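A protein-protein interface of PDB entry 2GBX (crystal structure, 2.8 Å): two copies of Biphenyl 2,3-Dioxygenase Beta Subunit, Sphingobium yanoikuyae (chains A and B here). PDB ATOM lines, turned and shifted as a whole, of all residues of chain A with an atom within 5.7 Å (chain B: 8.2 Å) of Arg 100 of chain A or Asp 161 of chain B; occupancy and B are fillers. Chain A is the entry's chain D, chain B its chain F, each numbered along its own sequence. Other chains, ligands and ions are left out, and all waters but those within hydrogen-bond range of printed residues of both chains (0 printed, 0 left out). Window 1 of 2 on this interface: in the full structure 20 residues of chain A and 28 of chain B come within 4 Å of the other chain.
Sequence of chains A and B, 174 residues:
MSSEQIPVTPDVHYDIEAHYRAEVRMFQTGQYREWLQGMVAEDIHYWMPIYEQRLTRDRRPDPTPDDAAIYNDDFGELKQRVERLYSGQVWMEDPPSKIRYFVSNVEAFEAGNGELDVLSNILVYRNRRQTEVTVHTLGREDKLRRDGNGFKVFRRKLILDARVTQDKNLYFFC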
ATOM      1  N   GLN A  28      -0.473  20.106  -1.098  1.00  0.00           N
ATOM      2  CA  GLN A  28      -0.194  18.814  -1.729  1.00  0.00           C
ATOM      3  C   GLN A  28       0.976  18.886  -2.710  1.00  0.00           C
ATOM      4  O   GLN A  28       1.816  17.983  -2.745  1.00  0.00           O
ATOM      5  CB  GLN A  28      -1.446  18.287  -2.439  1.00  0.00           C
ATOM      6  CG  GLN A  28      -2.593  17.951  -1.488  1.00  0.00           C
ATOM      7  CD  GLN A  28      -3.868  17.520  -2.200  1.00  0.00           C
ATOM      8  OE1 GLN A  28      -4.901  17.313  -1.561  1.00  0.00           O
ATOM      9  NE2 GLN A  28      -3.802  17.380  -3.521  1.00  0.00           N
ATOM     10  N   LYS A  98       3.556  11.814   0.937  1.00  0.00           N
ATOM     11  CA  LYS A  98       2.355  12.207   0.241  1.00  0.00           C
ATOM     12  C   LYS A  98       1.285  12.640   1.223  1.00  0.00           C
ATOM     13  O   LYS A  98       1.094  12.008   2.242  1.00  0.00           O
ATOM     14  CB  LYS A  98       1.852  11.043  -0.584  1.00  0.00           C
ATOM     15  CG  LYS A  98       2.695  10.743  -1.774  1.00  0.00           C
ATOM     16  CD  LYS A  98       1.901  10.965  -3.021  1.00  0.00           C
ATOM     17  CE  LYS A  98       2.129   9.876  -4.029  1.00  0.00           C
ATOM     18  NZ  LYS A  98       1.075   9.913  -5.069  1.00  0.00           N
ATOM     19  N   ILE A  99       0.581  13.717   0.916  1.00  0.00           N
ATOM     20  CA  ILE A  99      -0.540  14.125   1.758  1.00  0.00           C
ATOM     21  C   ILE A  99      -1.731  14.453   0.860  1.00  0.00           C
ATOM     22  O   ILE A  99      -1.553  14.865  -0.288  1.00  0.00           O
ATOM     23  CB  ILE A  99      -0.168  15.344   2.638  1.00  0.00           C
ATOM     24  CG1 ILE A  99      -1.268  15.631   3.665  1.00  0.00           C
ATOM     25  CG2 ILE A  99       0.099  16.573   1.777  1.00  0.00           C
ATOM     26  CD1 ILE A  99      -0.837  16.570   4.768  1.00  0.00           C
ATOM     27  N   ARG A 100      -2.941  14.252   1.378  1.00  0.00           N
ATOM     28  CA  ARG A 100      -4.158  14.503   0.609  1.00  0.00           C
ATOM     29  C   ARG A 100      -5.298  14.939   1.526  1.00  0.00           C
ATOM     30  O   ARG A 100      -5.725  14.184   2.403  1.00  0.00           O
ATOM     31  CB  ARG A 100      -4.549  13.251  -0.180  1.00  0.00           C
ATOM     32  CG  ARG A 100      -5.535  13.509  -1.313  1.00  0.00           C
ATOM     33  CD  ARG A 100      -5.499  12.390  -2.346  1.00  0.00           C
ATOM     34  NE  ARG A 100      -4.266  12.410  -3.136  1.00  0.00           N
ATOM     35  CZ  ARG A 100      -4.061  13.155  -4.222  1.00  0.00           C
ATOM     36  NH1 ARG A 100      -5.000  13.978  -4.683  1.00  0.00           N
ATOM     37  NH2 ARG A 100      -2.895  13.081  -4.855  1.00  0.00           N
ATOM     38  N   TYR A 101      -5.783  16.161   1.313  1.00  0.00           N
ATOM     39  CA  TYR A 101      -6.840  16.741   2.139  1.00  0.00           C
ATOM     40  C   TYR A 101      -8.204  16.513   1.498  1.00  0.00           C
ATOM     41  O   TYR A 101      -8.319  16.435   0.273  1.00  0.00           O
ATOM     42  CB  TYR A 101      -6.613  18.244   2.321  1.00  0.00           C
ATOM     43  CG  TYR A 101      -5.286  18.610   2.950  1.00  0.00           C
ATOM     44  CD1 TYR A 101      -5.192  18.888   4.313  1.00  0.00           C
ATOM     45  CD2 TYR A 101      -4.124  18.688   2.182  1.00  0.00           C
ATOM     46  CE1 TYR A 101      -3.976  19.229   4.895  1.00  0.00           C
ATOM     47  CE2 TYR A 101      -2.904  19.027   2.755  1.00  0.00           C
ATOM     48  CZ  TYR A 101      -2.838  19.296   4.111  1.00  0.00           C
ATOM     49  OH  TYR A 101      -1.632  19.634   4.684  1.00  0.00           O
ATOM     50  N   PHE A 102      -9.231  16.407   2.337  1.00  0.00           N
ATOM     51  CA  PHE A 102     -10.613  16.298   1.878  1.00  0.00           C
ATOM     52  C   PHE A 102     -11.489  17.262   2.671  1.00  0.00           C
ATOM     53  O   PHE A 102     -12.141  16.874   3.644  1.00  0.00           O
ATOM     54  CB  PHE A 102     -11.114  14.859   2.015  1.00  0.00           C
ATOM     55  CG  PHE A 102     -10.462  13.901   1.059  1.00  0.00           C
ATOM     56  CD1 PHE A 102     -11.024  13.654  -0.186  1.00  0.00           C
ATOM     57  CD2 PHE A 102      -9.281  13.255   1.400  1.00  0.00           C
ATOM     58  CE1 PHE A 102     -10.423  12.772  -1.076  1.00  0.00           C
ATOM     59  CE2 PHE A 102      -8.673  12.371   0.517  1.00  0.00           C
ATOM     60  CZ  PHE A 102      -9.244  12.131  -0.724  1.00  0.00           C
ATOM     61  N   LEU A 123     -10.254  16.290   6.489  1.00  0.00           N
ATOM     62  CA  LEU A 123      -9.767  14.917   6.620  1.00  0.00           C
ATOM     63  C   LEU A 123      -8.442  14.767   5.874  1.00  0.00           C
ATOM     64  O   LEU A 123      -8.415  14.754   4.641  1.00  0.00           O
ATOM     65  CB  LEU A 123     -10.802  13.930   6.067  1.00  0.00           C
ATOM     66  CG  LEU A 123     -10.387  12.460   5.921  1.00  0.00           C
ATOM     67  CD1 LEU A 123      -9.829  11.913   7.228  1.00  0.00           C
ATOM     68  CD2 LEU A 123     -11.569  11.624   5.452  1.00  0.00           C
ATOM     69  N   VAL A 124      -7.351  14.656   6.630  1.00  0.00           N
ATOM     70  CA  VAL A 124      -6.010  14.545   6.059  1.00  0.00           C
ATOM     71  C   VAL A 124      -5.576  13.082   5.976  1.00  0.00           C
ATOM     72  O   VAL A 124      -5.572  12.373   6.984  1.00  0.00           O
ATOM     73  CB  VAL A 124      -4.978  15.322   6.903  1.00  0.00           C
ATOM     74  CG1 VAL A 124      -3.604  15.274   6.247  1.00  0.00           C
ATOM     75  CG2 VAL A 124      -5.426  16.763   7.100  1.00  0.00           C
ATOM     76  N   TYR A 125      -5.214  12.645   4.771  1.00  0.00           N
ATOM     77  CA  TYR A 125      -4.687  11.299   4.540  1.00  0.00           C
ATOM     78  C   TYR A 125      -3.224  11.380   4.110  1.00  0.00           C
ATOM     79  O   TYR A 125      -2.910  11.968   3.073  1.00  0.00           O
ATOM     80  CB  TYR A 125      -5.505  10.572   3.467  1.00  0.00           C
ATOM     81  CG  TYR A 125      -6.421   9.498   4.010  1.00  0.00           C
ATOM     82  CD1 TYR A 125      -5.970   8.189   4.164  1.00  0.00           C
ATOM     83  CD2 TYR A 125      -7.738   9.785   4.361  1.00  0.00           C
ATOM     84  CE1 TYR A 125      -6.803   7.194   4.657  1.00  0.00           C
ATOM     85  CE2 TYR A 125      -8.581   8.797   4.857  1.00  0.00           C
ATOM     86  CZ  TYR A 125      -8.107   7.503   5.002  1.00  0.00           C
ATOM     87  OH  TYR A 125      -8.937   6.521   5.492  1.00  0.00           O
ATOM     88  N   ARG A 126      -2.341  10.785   4.910  1.00  0.00           N
ATOM     89  CA  ARG A 126      -0.901  10.842   4.670  1.00  0.00           C
ATOM     90  C   ARG A 126      -0.349   9.458   4.334  1.00  0.00           C
ATOM     91  O   ARG A 126      -0.707   8.470   4.976  1.00  0.00           O
ATOM     92  CB  ARG A 126      -0.181  11.384   5.905  1.00  0.00           C
ATOM     93  CG  ARG A 126      -0.721  12.713   6.415  1.00  0.00           C
ATOM     94  CD  ARG A 126       0.027  13.170   7.654  1.00  0.00           C
ATOM     95  NE  ARG A 126       1.419  13.509   7.364  1.00  0.00           N
ATOM     96  CZ  ARG A 126       2.314  13.887   8.275  1.00  0.00           C
ATOM     97  NH1 ARG A 126       1.979  13.978   9.558  1.00  0.00           N
ATOM     98  NH2 ARG A 126       3.556  14.173   7.901  1.00  0.00           N
ATOM     99  N   ASN A 127       0.516   9.400   3.323  1.00  0.00           N
ATOM    100  CA  ASN A 127       1.188   8.162   2.929  1.00  0.00           C
ATOM    101  C   ASN A 127       2.683   8.393   2.726  1.00  0.00           C
ATOM    102  O   ASN A 127       3.091   9.425   2.189  1.00  0.00           O
ATOM    103  CB  ASN A 127       0.578   7.604   1.640  1.00  0.00           C
ATOM    104  CG  ASN A 127      -0.815   7.035   1.846  1.00  0.00           C
ATOM    105  OD1 ASN A 127      -1.745   7.753   2.210  1.00  0.00           O
ATOM    106  ND2 ASN A 127      -0.965   5.738   1.601  1.00  0.00           N
ATOM    107  N   TYR B  51       4.395   4.830  -9.777  1.00  0.00           N
ATOM    108  CA  TYR B  51       5.436   5.670  -9.189  1.00  0.00           C
ATOM    109  C   TYR B  51       6.223   4.863  -8.162  1.00  0.00           C
ATOM    110  O   TYR B  51       5.644   4.063  -7.424  1.00  0.00           O
ATOM    111  CB  TYR B  51       4.832   6.904  -8.513  1.00  0.00           C
ATOM    112  CG  TYR B  51       4.297   7.938  -9.478  1.00  0.00           C
ATOM    113  CD1 TYR B  51       5.128   8.929  -9.994  1.00  0.00           C
ATOM    114  CD2 TYR B  51       2.961   7.932  -9.867  1.00  0.00           C
ATOM    115  CE1 TYR B  51       4.643   9.886 -10.878  1.00  0.00           C
ATOM    116  CE2 TYR B  51       2.466   8.885 -10.751  1.00  0.00           C
ATOM    117  CZ  TYR B  51       3.311   9.857 -11.253  1.00  0.00           C
ATOM    118  OH  TYR B  51       2.826  10.801 -12.128  1.00  0.00           O
ATOM    119  N   GLN B  53       9.492   4.963  -5.065  1.00  0.00           N
ATOM    120  CA  GLN B  53      10.168   5.818  -4.096  1.00  0.00           C
ATOM    121  C   GLN B  53      11.618   6.034  -4.523  1.00  0.00           C
ATOM    122  O   GLN B  53      12.432   5.111  -4.473  1.00  0.00           O
ATOM    123  CB  GLN B  53      10.119   5.202  -2.692  1.00  0.00           C
ATOM    124  CG  GLN B  53       8.714   4.914  -2.158  1.00  0.00           C
ATOM    125  CD  GLN B  53       7.911   6.173  -1.874  1.00  0.00           C
ATOM    126  OE1 GLN B  53       7.530   6.903  -2.789  1.00  0.00           O
ATOM    127  NE2 GLN B  53       7.638   6.423  -0.600  1.00  0.00           N
ATOM    128  N   SER B 104     -13.341  15.255  -4.046  1.00  0.00           N
ATOM    129  CA  SER B 104     -13.054  16.555  -3.438  1.00  0.00           C
ATOM    130  C   SER B 104     -12.009  17.323  -4.248  1.00  0.00           C
ATOM    131  O   SER B 104     -11.321  16.747  -5.090  1.00  0.00           O
ATOM    132  CB  SER B 104     -12.564  16.369  -2.000  1.00  0.00           C
ATOM    133  OG  SER B 104     -12.378  17.618  -1.355  1.00  0.00           O
ATOM    134  N   ASN B 105     -11.902  18.624  -3.977  1.00  0.00           N
ATOM    135  CA  ASN B 105     -10.953  19.507  -4.666  1.00  0.00           C
ATOM    136  C   ASN B 105     -11.092  19.488  -6.193  1.00  0.00           C
ATOM    137  O   ASN B 105     -10.101  19.370  -6.919  1.00  0.00           O
ATOM    138  CB  ASN B 105      -9.509  19.194  -4.237  1.00  0.00           C
ATOM    139  CG  ASN B 105      -9.040  20.065  -3.090  1.00  0.00           C
ATOM    140  OD1 ASN B 105      -9.672  20.123  -2.036  1.00  0.00           O
ATOM    141  ND2 ASN B 105      -7.923  20.753  -3.295  1.00  0.00           N
ATOM    142  N   LEU B 119      -8.395  18.798 -12.096  1.00  0.00           N
ATOM    143  CA  LEU B 119      -7.728  18.109 -10.990  1.00  0.00           C
ATOM    144  C   LEU B 119      -8.769  17.734  -9.937  1.00  0.00           C
ATOM    145  O   LEU B 119      -9.757  18.450  -9.759  1.00  0.00           O
ATOM    146  CB  LEU B 119      -6.664  19.013 -10.361  1.00  0.00           C
ATOM    147  CG  LEU B 119      -5.624  19.615 -11.310  1.00  0.00           C
ATOM    148  CD1 LEU B 119      -4.701  20.561 -10.554  1.00  0.00           C
ATOM    149  CD2 LEU B 119      -4.822  18.522 -12.000  1.00  0.00           C
ATOM    150  N   SER B 120      -8.549  16.619  -9.243  1.00  0.00           N
ATOM    151  CA  SER B 120      -9.507  16.137  -8.243  1.00  0.00           C
ATOM    152  C   SER B 120      -8.891  15.143  -7.255  1.00  0.00           C
ATOM    153  O   SER B 120      -8.049  14.324  -7.628  1.00  0.00           O
ATOM    154  CB  SER B 120     -10.707  15.489  -8.939  1.00  0.00           C
ATOM    155  OG  SER B 120     -11.675  15.054  -7.998  1.00  0.00           O
ATOM    156  N   ASN B 121      -9.327  15.231  -5.999  1.00  0.00           N
ATOM    157  CA  ASN B 121      -8.950  14.277  -4.955  1.00  0.00           C
ATOM    158  C   ASN B 121     -10.066  13.254  -4.768  1.00  0.00           C
ATOM    159  O   ASN B 121     -11.246  13.614  -4.775  1.00  0.00           O
ATOM    160  CB  ASN B 121      -8.707  15.005  -3.629  1.00  0.00           C
ATOM    161  CG  ASN B 121      -7.635  16.077  -3.733  1.00  0.00           C
ATOM    162  OD1 ASN B 121      -7.083  16.323  -4.807  1.00  0.00           O
ATOM    163  ND2 ASN B 121      -7.338  16.722  -2.611  1.00  0.00           N
ATOM    164  N   ILE B 122      -9.695  11.985  -4.600  1.00  0.00           N
ATOM    165  CA  ILE B 122     -10.669  10.896  -4.484  1.00  0.00           C
ATOM    166  C   ILE B 122     -10.332   9.959  -3.324  1.00  0.00           C
ATOM    167  O   ILE B 122      -9.192   9.507  -3.194  1.00  0.00           O
ATOM    168  CB  ILE B 122     -10.742  10.063  -5.784  1.00  0.00           C
ATOM    169  CG1 ILE B 122     -11.077  10.956  -6.984  1.00  0.00           C
ATOM    170  CG2 ILE B 122     -11.778   8.952  -5.649  1.00  0.00           C
ATOM    171  CD1 ILE B 122     -11.253  10.197  -8.284  1.00  0.00           C
ATOM    172  N   LEU B 123     -11.333   9.675  -2.490  1.00  0.00           N
ATOM    173  CA  LEU B 123     -11.211   8.699  -1.406  1.00  0.00           C
ATOM    174  C   LEU B 123     -12.222   7.578  -1.631  1.00  0.00           C
ATOM    175  O   LEU B 123     -13.433   7.813  -1.602  1.00  0.00           O
ATOM    176  CB  LEU B 123     -11.464   9.368  -0.050  1.00  0.00           C
ATOM    177  CG  LEU B 123     -11.381   8.486   1.201  1.00  0.00           C
ATOM    178  CD1 LEU B 123     -10.006   7.849   1.328  1.00  0.00           C
ATOM    179  CD2 LEU B 123     -11.711   9.299   2.443  1.00  0.00           C
ATOM    180  N   HIS B 136      -8.606   3.654  -0.140  1.00  0.00           N
ATOM    181  CA  HIS B 136      -7.673   4.101  -1.177  1.00  0.00           C
ATOM    182  C   HIS B 136      -7.797   5.601  -1.432  1.00  0.00           C
ATOM    183  O   HIS B 136      -8.827   6.070  -1.920  1.00  0.00           O
ATOM    184  CB  HIS B 136      -7.925   3.350  -2.488  1.00  0.00           C
ATOM    185  CG  HIS B 136      -7.645   1.882  -2.408  1.00  0.00           C
ATOM    186  ND1 HIS B 136      -6.368   1.373  -2.297  1.00  0.00           N
ATOM    187  CD2 HIS B 136      -8.477   0.813  -2.437  1.00  0.00           C
ATOM    188  CE1 HIS B 136      -6.427   0.053  -2.253  1.00  0.00           C
ATOM    189  NE2 HIS B 136      -7.695  -0.312  -2.337  1.00  0.00           N
ATOM    190  N   THR B 137      -6.744   6.345  -1.098  1.00  0.00           N
ATOM    191  CA  THR B 137      -6.647   7.760  -1.453  1.00  0.00           C
ATOM    192  C   THR B 137      -5.979   7.875  -2.821  1.00  0.00           C
ATOM    193  O   THR B 137      -4.988   7.194  -3.089  1.00  0.00           O
ATOM    194  CB  THR B 137      -5.835   8.551  -0.414  1.00  0.00           C
ATOM    195  OG1 THR B 137      -4.565   7.919  -0.209  1.00  0.00           O
ATOM    196  CG2 THR B 137      -6.584   8.614   0.902  1.00  0.00           C
ATOM    197  N   LEU B 138      -6.524   8.736  -3.678  1.00  0.00           N
ATOM    198  CA  LEU B 138      -6.083   8.822  -5.070  1.00  0.00           C
ATOM    199  C   LEU B 138      -6.234  10.236  -5.630  1.00  0.00           C
ATOM    200  O   LEU B 138      -7.189  10.944  -5.304  1.00  0.00           O
ATOM    201  CB  LEU B 138      -6.885   7.830  -5.920  1.00  0.00           C
ATOM    202  CG  LEU B 138      -6.485   7.646  -7.388  1.00  0.00           C
ATOM    203  CD1 LEU B 138      -6.864   6.254  -7.876  1.00  0.00           C
ATOM    204  CD2 LEU B 138      -7.115   8.709  -8.279  1.00  0.00           C
ATOM    205  N   GLY B 139      -5.279  10.633  -6.473  1.00  0.00           N
ATOM    206  CA  GLY B 139      -5.314  11.924  -7.160  1.00  0.00           C
ATOM    207  C   GLY B 139      -5.639  11.736  -8.630  1.00  0.00           C
ATOM    208  O   GLY B 139      -5.016  10.916  -9.307  1.00  0.00           O
ATOM    209  N   ARG B 140      -6.613  12.499  -9.125  1.00  0.00           N
ATOM    210  CA  ARG B 140      -7.105  12.355 -10.494  1.00  0.00           C
ATOM    211  C   ARG B 140      -6.775  13.591 -11.332  1.00  0.00           C
ATOM    212  O   ARG B 140      -6.941  14.722 -10.873  1.00  0.00           O
ATOM    213  CB  ARG B 140      -8.618  12.118 -10.474  1.00  0.00           C
ATOM    214  CG  ARG B 140      -9.237  11.857 -11.839  1.00  0.00           C
ATOM    215  CD  ARG B 140     -10.664  11.339 -11.714  1.00  0.00           C
ATOM    216  NE  ARG B 140     -11.547  12.299 -11.052  1.00  0.00           N
ATOM    217  CZ  ARG B 140     -12.840  12.094 -10.804  1.00  0.00           C
ATOM    218  NH1 ARG B 140     -13.433  10.959 -11.166  1.00  0.00           N
ATOM    219  NH2 ARG B 140     -13.551  13.036 -10.192  1.00  0.00           N
ATOM    220  N   GLU B 141      -6.302  13.359 -12.556  1.00  0.00           N
ATOM    221  CA  GLU B 141      -5.999  14.429 -13.509  1.00  0.00           C
ATOM    222  C   GLU B 141      -6.619  14.087 -14.864  1.00  0.00           C
ATOM    223  O   GLU B 141      -6.190  13.139 -15.524  1.00  0.00           O
ATOM    224  CB  GLU B 141      -4.486  14.601 -13.660  1.00  0.00           C
ATOM    225  CG  GLU B 141      -3.765  14.950 -12.365  1.00  0.00           C
ATOM    226  CD  GLU B 141      -2.281  15.218 -12.564  1.00  0.00           C
ATOM    227  OE1 GLU B 141      -1.742  14.883 -13.641  1.00  0.00           O
ATOM    228  OE2 GLU B 141      -1.649  15.767 -11.635  1.00  0.00           O
ATOM    229  N   LEU B 158      -4.543   8.598 -13.120  1.00  0.00           N
ATOM    230  CA  LEU B 158      -4.800   8.324 -11.706  1.00  0.00           C
ATOM    231  C   LEU B 158      -3.485   8.135 -10.956  1.00  0.00           C
ATOM    232  O   LEU B 158      -2.660   7.307 -11.342  1.00  0.00           O
ATOM    233  CB  LEU B 158      -5.663   7.068 -11.558  1.00  0.00           C
ATOM    234  CG  LEU B 158      -7.041   7.110 -12.224  1.00  0.00           C
ATOM    235  CD1 LEU B 158      -7.689   5.734 -12.196  1.00  0.00           C
ATOM    236  CD2 LEU B 158      -7.937   8.141 -11.555  1.00  0.00           C
ATOM    237  N   ILE B 159      -3.300   8.904  -9.884  1.00  0.00           N
ATOM    238  CA  ILE B 159      -2.080   8.853  -9.079  1.00  0.00           C
ATOM    239  C   ILE B 159      -2.375   8.259  -7.701  1.00  0.00           C
ATOM    240  O   ILE B 159      -3.012   8.903  -6.864  1.00  0.00           O
ATOM    241  CB  ILE B 159      -1.459  10.259  -8.901  1.00  0.00           C
ATOM    242  CG1 ILE B 159      -1.116  10.879 -10.261  1.00  0.00           C
ATOM    243  CG2 ILE B 159      -0.208  10.188  -8.034  1.00  0.00           C
ATOM    244  CD1 ILE B 159      -2.301  11.503 -10.974  1.00  0.00           C
ATOM    245  N   LEU B 160      -1.911   7.032  -7.476  1.00  0.00           N
ATOM    246  CA  LEU B 160      -2.087   6.358  -6.186  1.00  0.00           C
ATOM    247  C   LEU B 160      -1.091   6.891  -5.161  1.00  0.00           C
ATOM    248  O   LEU B 160       0.071   7.143  -5.487  1.00  0.00           O
ATOM    249  CB  LEU B 160      -1.929   4.838  -6.333  1.00  0.00           C
ATOM    250  CG  LEU B 160      -3.182   4.065  -6.756  1.00  0.00           C
ATOM    251  CD1 LEU B 160      -3.883   4.737  -7.928  1.00  0.00           C
ATOM    252  CD2 LEU B 160      -2.829   2.622  -7.093  1.00  0.00           C
ATOM    253  N   ASP B 161      -1.552   7.053  -3.924  1.00  0.00           N
ATOM    254  CA  ASP B 161      -0.719   7.593  -2.851  1.00  0.00           C
ATOM    255  C   ASP B 161       0.203   6.524  -2.280  1.00  0.00           C
ATOM    256  O   ASP B 161       1.423   6.704  -2.237  1.00  0.00           O
ATOM    257  CB  ASP B 161      -1.589   8.172  -1.731  1.00  0.00           C
ATOM    258  CG  ASP B 161      -2.446   9.339  -2.191  1.00  0.00           C
ATOM    259  OD1 ASP B 161      -2.440   9.655  -3.409  1.00  0.00           O
ATOM    260  OD2 ASP B 161      -3.129   9.940  -1.327  1.00  0.00           O
ATOM    261  N   ALA B 162      -0.388   5.414  -1.842  1.00  0.00           N
ATOM    262  CA  ALA B 162       0.367   4.312  -1.253  1.00  0.00           C
ATOM    263  C   ALA B 162       1.148   3.556  -2.325  1.00  0.00           C
ATOM    264  O   ALA B 162       0.625   3.289  -3.410  1.00  0.00           O
ATOM    265  CB  ALA B 162      -0.569   3.363  -0.517  1.00  0.00           C
ATOM    266  N   ARG B 163       2.398   3.217  -2.015  1.00  0.00           N
ATOM    267  CA  ARG B 163       3.242   2.453  -2.930  1.00  0.00           C
ATOM    268  C   ARG B 163       2.780   1.000  -2.963  1.00  0.00           C
ATOM    269  O   ARG B 163       2.452   0.469  -4.025  1.00  0.00           O
ATOM    270  CB  ARG B 163       4.714   2.538  -2.503  1.00  0.00           C
ATOM    271  CG  ARG B 163       5.691   1.766  -3.393  1.00  0.00           C
ATOM    272  CD  ARG B 163       5.683   2.277  -4.826  1.00  0.00           C
ATOM    273  NE  ARG B 163       6.671   1.594  -5.660  1.00  0.00           N
ATOM    274  CZ  ARG B 163       6.483   0.427  -6.277  1.00  0.00           C
ATOM    275  NH1 ARG B 163       5.334  -0.235  -6.167  1.00  0.00           N
ATOM    276  NH2 ARG B 163       7.463  -0.085  -7.012  1.00  0.00           N
ATOM    277  N   VAL B 164       2.760   0.369  -1.791  1.00  0.00           N
ATOM    278  CA  VAL B 164       2.265  -0.996  -1.652  1.00  0.00           C
ATOM    279  C   VAL B 164       0.755  -0.957  -1.431  1.00  0.00           C
ATOM    280  O   VAL B 164       0.284  -0.418  -0.427  1.00  0.00           O
ATOM    281  CB  VAL B 164       2.939  -1.728  -0.474  1.00  0.00           C
ATOM    282  CG1 VAL B 164       2.404  -3.148  -0.349  1.00  0.00           C
ATOM    283  CG2 VAL B 164       4.449  -1.741  -0.653  1.00  0.00           C
ATOM    284  N   THR B 165       0.004  -1.524  -2.372  1.00  0.00           N
ATOM    285  CA  THR B 165      -1.456  -1.511  -2.317  1.00  0.00           C
ATOM    286  C   THR B 165      -1.972  -2.465  -1.239  1.00  0.00           C
ATOM    287  O   THR B 165      -1.887  -3.685  -1.389  1.00  0.00           O
ATOM    288  CB  THR B 165      -2.072  -1.903  -3.677  1.00  0.00           C
ATOM    289  OG1 THR B 165      -1.558  -1.046  -4.705  1.00  0.00           O
ATOM    290  CG2 THR B 165      -3.590  -1.789  -3.638  1.00  0.00           C
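OE1 of Gln 28 of chain A sits at hydrogen-bond distance from ND2 of Asn 121 of chain B.
NZ of Lys 98 of chain A lies within hydrogen-bond range of O of Leu 160 of chain B (3.0 Å).
The side-chain amino group of Lys 98 of chain A lies within salt-bridge range of the side-chain carboxylate of Asp 161 of chain B (3.9 Å).
OD1 of Asn 121 of chain B sits at hydrogen-bond distance from NH1 of Arg 100 of chain A.
NE of Arg 100 of chain A is in salt-bridge range of OD2 of Asp 161 of chain B (3.3 Å).
ND2 of Asn 121 of chain B is in hydrogen-bond range of O of Tyr 101 of chain A (3.1 Å).
The backbone NH (N) of Lys 98 of chain A lies within hydrogen-bond range of the backbone carbonyl oxygen (O) of Asn 127 of chain A, at 2.7 Å.
The backbone NH (N) of Arg 100 of chain A sits at hydrogen-bond distance from the backbone carbonyl oxygen (O) of Tyr 125 of chain A (2.8 Å).
The side-chain hydroxyl (OG) of Ser 120 of chain B sits at hydrogen-bond distance from the backbone carbonyl oxygen (O) of Ser 104 of chain B.
The backbone NH of Asn 121 of chain B sits at hydrogen-bond distance from the backbone carbonyl oxygen of Ser 104 of chain B (2.7 Å).
The side-chain hydroxyl (OG1) of Thr 137 of chain B sits at hydrogen-bond distance from the side-chain carboxylate (OD2) of Asp 161 of chain B, at 2.7 Å.
O of Gly 139 of chain B lies within hydrogen-bond range of N of Ile 159 of chain B (2.7 Å).
Ile 159 of chain B touches Lys 98 of chain A (CG2 to NZ, 3.2 Å).
Arg 100 of chain A touches Leu 138 of chain B.
CD1 of Phe 102 of chain A touches CB of Ser 104 of chain B (3.6 Å).
Asn 121 of chain B touches Phe 102 of chain A.
Leu 123 of chain B touches Phe 102 of chain A.
Leu 123 of chain A touches Leu 123 of chain B (CD2 to CD2, 3.8 Å).
Tyr 125 of chain A touches Leu 123 of chain B.
CG of Tyr 125 of chain A touches CG2 of Thr 137 of chain B (3.2 Å).
Asp 161 of chain B touches Asn 127 of chain A.
CB of Ala 162 of chain B touches ND2 of Asn 127 of chain A, at 3.2 Å.
Of the printed residues of chain B, Phe 102 of chain A touches Ser 104 (3.6 Å), Asn 121 (3.7 Å), Ile 122 (3.6 Å) and Leu 123 (3.5 Å).
Val 124 of chain A touches none of the printed residues of chain B.
Of chain A, only Lys 98 (3.7 Å), Arg 100 (3.3 Å) and Asn 127 (3.8 Å) come within 4 Å of Asp 161 of chain B.
Of the printed residues of chain A, Ala 162 of chain B touches Asn 127 (3.2 Å).
Thr 165 of chain B touches none of the printed residues of chain A.
The nearest printed residue of chain B that does not touch Lys 98 of chain A is Tyr 51 of chain B (5.5 Å).
Of the 23 printed residues of chain B, 11 touch a printed residue of chain A.
Hydrophobic or aromatic side chains of chain B within 4 Å of the printed part of chain A: Leu 123, Ile 159 and Ala 162.
Along chain B the printed residues that touch a printed residue of chain A span positions 104 to 162.
Among the printed residues, 19 pairs touch across the chains.
Leu 123 of chain A touches its own counterpart, Leu 123 of chain B.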
